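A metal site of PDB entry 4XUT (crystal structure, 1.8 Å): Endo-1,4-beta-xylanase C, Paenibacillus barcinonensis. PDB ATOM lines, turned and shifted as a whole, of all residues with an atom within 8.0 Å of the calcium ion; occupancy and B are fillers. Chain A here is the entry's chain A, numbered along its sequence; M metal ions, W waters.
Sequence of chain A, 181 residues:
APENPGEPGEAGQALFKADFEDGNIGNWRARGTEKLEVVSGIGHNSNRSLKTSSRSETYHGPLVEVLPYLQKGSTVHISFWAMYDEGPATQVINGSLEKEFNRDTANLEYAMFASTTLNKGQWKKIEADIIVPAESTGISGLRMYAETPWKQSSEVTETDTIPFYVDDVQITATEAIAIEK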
ATOM      1  N   ALA A  18       2.590   9.080 -14.894  1.00  0.00           N
ATOM      2  CA  ALA A  18       3.577   9.919 -14.211  1.00  0.00           C
ATOM      3  C   ALA A  18       2.904  10.866 -13.222  1.00  0.00           C
ATOM      4  O   ALA A  18       2.157  11.752 -13.624  1.00  0.00           O
ATOM      5  CB  ALA A  18       4.409  10.699 -15.222  1.00  0.00           C
ATOM      6  N   ASP A  19       3.194  10.674 -11.925  1.00  0.00           N
ATOM      7  CA  ASP A  19       2.676  11.570 -10.867  1.00  0.00           C
ATOM      8  C   ASP A  19       3.773  12.365 -10.122  1.00  0.00           C
ATOM      9  O   ASP A  19       3.467  13.237  -9.305  1.00  0.00           O
ATOM     10  CB  ASP A  19       1.783  10.808  -9.890  1.00  0.00           C
ATOM     11  CG  ASP A  19       2.539   9.720  -9.098  1.00  0.00           C
ATOM     12  OD1 ASP A  19       3.776   9.754  -8.989  1.00  0.00           O
ATOM     13  OD2 ASP A  19       1.870   8.823  -8.605  1.00  0.00           O
ATOM     14  N   PHE A  20       5.028  12.074 -10.467  1.00  0.00           N
ATOM     15  CA  PHE A  20       6.227  12.768  -9.973  1.00  0.00           C
ATOM     16  C   PHE A  20       6.436  12.709  -8.458  1.00  0.00           C
ATOM     17  O   PHE A  20       7.289  13.410  -7.923  1.00  0.00           O
ATOM     18  CB  PHE A  20       6.208  14.213 -10.454  1.00  0.00           C
ATOM     19  CG  PHE A  20       6.093  14.317 -11.914  1.00  0.00           C
ATOM     20  CD1 PHE A  20       7.186  14.043 -12.721  1.00  0.00           C
ATOM     21  CD2 PHE A  20       4.873  14.598 -12.498  1.00  0.00           C
ATOM     22  CE1 PHE A  20       7.080  14.119 -14.095  1.00  0.00           C
ATOM     23  CE2 PHE A  20       4.757  14.659 -13.885  1.00  0.00           C
ATOM     24  CZ  PHE A  20       5.859  14.415 -14.665  1.00  0.00           C
ATOM     25  N   GLU A  21       5.691  11.826  -7.782  1.00  0.00           N
ATOM     26  CA  GLU A  21       5.714  11.770  -6.330  1.00  0.00           C
ATOM     27  C   GLU A  21       7.023  11.196  -5.789  1.00  0.00           C
ATOM     28  O   GLU A  21       7.412  11.519  -4.684  1.00  0.00           O
ATOM     29  CB  GLU A  21       4.499  11.031  -5.782  1.00  0.00           C
ATOM     30  CG  GLU A  21       3.177  11.773  -6.024  1.00  0.00           C
ATOM     31  CD  GLU A  21       3.211  13.214  -5.503  1.00  0.00           C
ATOM     32  OE1 GLU A  21       3.591  13.434  -4.322  1.00  0.00           O
ATOM     33  OE2 GLU A  21       2.906  14.162  -6.285  1.00  0.00           O
ATOM     34  N   ASP A  22       7.702  10.378  -6.595  1.00  0.00           N
ATOM     35  CA  ASP A  22       9.056   9.907  -6.286  1.00  0.00           C
ATOM     36  C   ASP A  22      10.161  10.969  -6.509  1.00  0.00           C
ATOM     37  O   ASP A  22      11.334  10.738  -6.219  1.00  0.00           O
ATOM     38  CB  ASP A  22       9.376   8.642  -7.089  1.00  0.00           C
ATOM     39  CG  ASP A  22       9.311   8.856  -8.617  1.00  0.00           C
ATOM     40  OD1 ASP A  22       9.112  10.002  -9.098  1.00  0.00           O
ATOM     41  OD2 ASP A  22       9.424   7.839  -9.335  1.00  0.00           O
ATOM     42  N   VAL A  38      11.411  18.792 -11.292  1.00  0.00           N
ATOM     43  CA  VAL A  38      10.362  18.247 -10.453  1.00  0.00           C
ATOM     44  C   VAL A  38      10.375  19.045  -9.155  1.00  0.00           C
ATOM     45  O   VAL A  38      11.384  19.083  -8.429  1.00  0.00           O
ATOM     46  CB  VAL A  38      10.508  16.732 -10.155  1.00  0.00           C
ATOM     47  CG1 VAL A  38       9.337  16.258  -9.291  1.00  0.00           C
ATOM     48  CG2 VAL A  38      10.523  15.946 -11.451  1.00  0.00           C
ATOM     49  N   VAL A  39       9.271  19.731  -8.893  1.00  0.00           N
ATOM     50  CA  VAL A  39       9.193  20.622  -7.733  1.00  0.00           C
ATOM     51  C   VAL A  39       8.431  19.941  -6.622  1.00  0.00           C
ATOM     52  O   VAL A  39       7.643  19.041  -6.854  1.00  0.00           O
ATOM     53  CB  VAL A  39       8.552  22.001  -8.063  1.00  0.00           C
ATOM     54  CG1 VAL A  39       9.411  22.771  -9.049  1.00  0.00           C
ATOM     55  CG2 VAL A  39       7.124  21.877  -8.555  1.00  0.00           C
ATOM     56  N   ILE A  42       4.064  21.831  -4.782  1.00  0.00           N
ATOM     57  CA  ILE A  42       3.111  22.208  -5.827  1.00  0.00           C
ATOM     58  C   ILE A  42       2.749  20.924  -6.600  1.00  0.00           C
ATOM     59  O   ILE A  42       3.644  20.216  -7.099  1.00  0.00           O
ATOM     60  CB  ILE A  42       3.679  23.205  -6.879  1.00  0.00           C
ATOM     61  CG1 ILE A  42       4.157  24.519  -6.248  1.00  0.00           C
ATOM     62  CG2 ILE A  42       2.631  23.479  -7.993  1.00  0.00           C
ATOM     63  CD1 ILE A  42       3.055  25.492  -5.893  1.00  0.00           C
ATOM     64  N   GLY A  43       1.467  20.630  -6.645  1.00  0.00           N
ATOM     65  CA  GLY A  43       0.999  19.433  -7.338  1.00  0.00           C
ATOM     66  C   GLY A  43      -0.513  19.391  -7.431  1.00  0.00           C
ATOM     67  O   GLY A  43      -1.222  20.147  -6.748  1.00  0.00           O
ATOM     68  N   HIS A  44      -1.007  18.508  -8.299  1.00  0.00           N
ATOM     69  CA  HIS A  44      -2.443  18.286  -8.451  1.00  0.00           C
ATOM     70  C   HIS A  44      -2.840  17.292  -7.355  1.00  0.00           C
ATOM     71  O   HIS A  44      -2.521  16.100  -7.450  1.00  0.00           O
ATOM     72  CB  HIS A  44      -2.819  17.744  -9.847  1.00  0.00           C
ATOM     73  CG  HIS A  44      -4.269  17.384  -9.986  1.00  0.00           C
ATOM     74  ND1 HIS A  44      -5.298  18.285  -9.770  1.00  0.00           N
ATOM     75  CD2 HIS A  44      -4.876  16.209 -10.306  1.00  0.00           C
ATOM     76  CE1 HIS A  44      -6.458  17.690  -9.978  1.00  0.00           C
ATOM     77  NE2 HIS A  44      -6.225  16.434 -10.295  1.00  0.00           N
ATOM     78  N   ASN A  45      -3.523  17.777  -6.325  1.00  0.00           N
ATOM     79  CA  ASN A  45      -3.908  16.942  -5.162  1.00  0.00           C
ATOM     80  C   ASN A  45      -2.770  16.057  -4.695  1.00  0.00           C
ATOM     81  O   ASN A  45      -2.915  14.842  -4.508  1.00  0.00           O
ATOM     82  CB  ASN A  45      -5.144  16.061  -5.467  1.00  0.00           C
ATOM     83  CG  ASN A  45      -6.368  16.852  -5.869  1.00  0.00           C
ATOM     84  OD1 ASN A  45      -7.162  16.394  -6.706  1.00  0.00           O
ATOM     85  ND2 ASN A  45      -6.565  18.034  -5.291  1.00  0.00           N
ATOM     86  N   SER A  46      -1.611  16.687  -4.579  1.00  0.00           N
ATOM     87  CA  SER A  46      -0.343  15.971  -4.380  1.00  0.00           C
ATOM     88  C   SER A  46       0.757  16.972  -4.142  1.00  0.00           C
ATOM     89  O   SER A  46       0.574  18.176  -4.326  1.00  0.00           O
ATOM     90  CB  SER A  46      -0.036  15.073  -5.598  1.00  0.00           C
ATOM     91  OG  SER A  46       0.439  15.809  -6.701  1.00  0.00           O
ATOM     92  N   ASN A  47       1.924  16.451  -3.773  1.00  0.00           N
ATOM     93  CA  ASN A  47       2.989  17.285  -3.311  1.00  0.00           C
ATOM     94  C   ASN A  47       3.994  17.644  -4.375  1.00  0.00           C
ATOM     95  O   ASN A  47       4.782  18.565  -4.179  1.00  0.00           O
ATOM     96  CB  ASN A  47       3.728  16.609  -2.153  1.00  0.00           C
ATOM     97  CG  ASN A  47       4.133  17.597  -1.080  1.00  0.00           C
ATOM     98  OD1 ASN A  47       4.914  18.505  -1.312  1.00  0.00           O
ATOM     99  ND2 ASN A  47       3.570  17.419   0.125  1.00  0.00           N
ATOM    100  N   ARG A  48       3.973  16.893  -5.479  1.00  0.00           N
ATOM    101  CA  ARG A  48       4.974  17.078  -6.511  1.00  0.00           C
ATOM    102  C   ARG A  48       4.403  17.126  -7.925  1.00  0.00           C
ATOM    103  O   ARG A  48       3.389  16.495  -8.221  1.00  0.00           O
ATOM    104  CB  ARG A  48       6.013  15.983  -6.445  1.00  0.00           C
ATOM    105  CG  ARG A  48       6.693  15.855  -5.090  1.00  0.00           C
ATOM    106  CD  ARG A  48       8.105  15.398  -5.291  1.00  0.00           C
ATOM    107  NE  ARG A  48       8.849  15.268  -4.047  1.00  0.00           N
ATOM    108  CZ  ARG A  48      10.165  15.432  -3.939  1.00  0.00           C
ATOM    109  NH1 ARG A  48      10.921  15.752  -4.999  1.00  0.00           N
ATOM    110  NH2 ARG A  48      10.728  15.291  -2.744  1.00  0.00           N
ATOM    111  N   SER A  49       5.114  17.875  -8.765  1.00  0.00           N
ATOM    112  CA  SER A  49       4.752  18.076 -10.173  1.00  0.00           C
ATOM    113  C   SER A  49       5.932  18.552 -10.981  1.00  0.00           C
ATOM    114  O   SER A  49       6.999  18.839 -10.436  1.00  0.00           O
ATOM    115  CB  SER A  49       3.592  19.042 -10.309  1.00  0.00           C
ATOM    116  OG  SER A  49       3.948  20.349  -9.859  1.00  0.00           O
ATOM    117  N   LEU A  50       5.772  18.568 -12.310  1.00  0.00           N
ATOM    118  CA  LEU A  50       6.867  18.870 -13.202  1.00  0.00           C
ATOM    119  C   LEU A  50       6.689  20.300 -13.671  1.00  0.00           C
ATOM    120  O   LEU A  50       5.707  20.612 -14.337  1.00  0.00           O
ATOM    121  CB  LEU A  50       6.845  17.925 -14.409  1.00  0.00           C
ATOM    122  CG  LEU A  50       7.882  18.197 -15.498  1.00  0.00           C
ATOM    123  CD1 LEU A  50       9.312  18.141 -14.952  1.00  0.00           C
ATOM    124  CD2 LEU A  50       7.704  17.186 -16.600  1.00  0.00           C
ATOM    125  N   TRP A 123      -5.821  23.981 -11.448  1.00  0.00           N
ATOM    126  CA  TRP A 123      -5.495  22.767 -12.218  1.00  0.00           C
ATOM    127  C   TRP A 123      -6.648  22.388 -13.142  1.00  0.00           C
ATOM    128  O   TRP A 123      -7.835  22.460 -12.760  1.00  0.00           O
ATOM    129  CB  TRP A 123      -5.155  21.608 -11.279  1.00  0.00           C
ATOM    130  CG  TRP A 123      -3.876  21.782 -10.571  1.00  0.00           C
ATOM    131  CD1 TRP A 123      -3.673  22.380  -9.349  1.00  0.00           C
ATOM    132  CD2 TRP A 123      -2.577  21.372 -11.035  1.00  0.00           C
ATOM    133  NE1 TRP A 123      -2.333  22.338  -9.019  1.00  0.00           N
ATOM    134  CE2 TRP A 123      -1.644  21.724 -10.032  1.00  0.00           C
ATOM    135  CE3 TRP A 123      -2.117  20.746 -12.198  1.00  0.00           C
ATOM    136  CZ2 TRP A 123      -0.264  21.492 -10.177  1.00  0.00           C
ATOM    137  CZ3 TRP A 123      -0.773  20.492 -12.336  1.00  0.00           C
ATOM    138  CH2 TRP A 123       0.151  20.857 -11.318  1.00  0.00           C
ATOM    139  N   VAL A 166       2.869  20.530 -15.020  1.00  0.00           N
ATOM    140  CA  VAL A 166       2.042  19.351 -15.369  1.00  0.00           C
ATOM    141  C   VAL A 166       2.142  18.248 -14.321  1.00  0.00           C
ATOM    142  O   VAL A 166       3.177  18.104 -13.638  1.00  0.00           O
ATOM    143  CB  VAL A 166       2.358  18.744 -16.767  1.00  0.00           C
ATOM    144  CG1 VAL A 166       2.167  19.795 -17.863  1.00  0.00           C
ATOM    145  CG2 VAL A 166       3.755  18.161 -16.827  1.00  0.00           C
ATOM    146  N   ASP A 167       1.088  17.463 -14.220  1.00  0.00           N
ATOM    147  CA  ASP A 167       1.007  16.391 -13.237  1.00  0.00           C
ATOM    148  C   ASP A 167       0.010  15.354 -13.706  1.00  0.00           C
ATOM    149  O   ASP A 167      -0.800  15.584 -14.613  1.00  0.00           O
ATOM    150  CB  ASP A 167       0.549  16.958 -11.873  1.00  0.00           C
ATOM    151  CG  ASP A 167       0.986  16.110 -10.677  1.00  0.00           C
ATOM    152  OD1 ASP A 167       1.651  15.062 -10.825  1.00  0.00           O
ATOM    153  OD2 ASP A 167       0.610  16.493  -9.523  1.00  0.00           O
ATOM    154  N   ASP A 168       0.065  14.194 -13.058  1.00  0.00           N
ATOM    155  CA  ASP A 168      -0.906  13.110 -13.236  1.00  0.00           C
ATOM    156  C   ASP A 168      -1.123  12.749 -14.711  1.00  0.00           C
ATOM    157  O   ASP A 168      -2.233  12.770 -15.229  1.00  0.00           O
ATOM    158  CB  ASP A 168      -2.224  13.429 -12.552  1.00  0.00           C
ATOM    159  CG  ASP A 168      -2.148  13.310 -11.035  1.00  0.00           C
ATOM    160  OD1 ASP A 168      -1.219  12.645 -10.525  1.00  0.00           O
ATOM    161  OD2 ASP A 168      -3.041  13.881 -10.368  1.00  0.00           O
ATOM    162  N   VAL A 169      -0.006  12.479 -15.364  1.00  0.00           N
ATOM    163  CA  VAL A 169       0.026  12.149 -16.795  1.00  0.00           C
ATOM    164  C   VAL A 169      -0.353  10.685 -16.872  1.00  0.00           C
ATOM    165  O   VAL A 169       0.180   9.879 -16.116  1.00  0.00           O
ATOM    166  CB  VAL A 169       1.407  12.409 -17.437  1.00  0.00           C
ATOM    167  CG1 VAL A 169       1.372  12.111 -18.929  1.00  0.00           C
ATOM    168  CG2 VAL A 169       1.845  13.848 -17.218  1.00  0.00           C
HETATM  169 CA    CA M   1       1.959  14.779  -8.396  1.00  0.00          CA
HETATM  170  O   HOH W   1       0.126  13.425  -8.294  1.00  0.00           O
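The backbone NH of Asn 47 sits at hydrogen-bond distance from the side-chain carboxylate of Glu 21.
The backbone NH of His 44 sits close to the side-chain carboxylate of Asp 167, at 2.9 Å.
The side-chain hydroxyl (OG) of Ser 46 sits close to the backbone carbonyl oxygen (O) of His 44, 3.1 Å away.
Along chain A the residues within 4 Å of the calcium ion span positions 19 to 167.
The nearest printed residue that does not touch the calcium ion is Asp 168 (4.4 Å).
The calcium ion is bound by O of Arg 48 (2.2 Å).
Water W1 is bound to the calcium ion, at 2.3 Å.
The backbone carbonyl oxygen (O) of Asp 19 binds the calcium ion (2.3 Å).
The calcium ion is bound by OE2 of Glu 21 (2.4 Å).
The side-chain carboxylate (OD2) of Asp 167 binds the calcium ion (2.5 Å).
OD1 of Asp 167 binds the calcium ion.
The calcium ion is bound by the side-chain hydroxyl (OG) of Ser 46.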
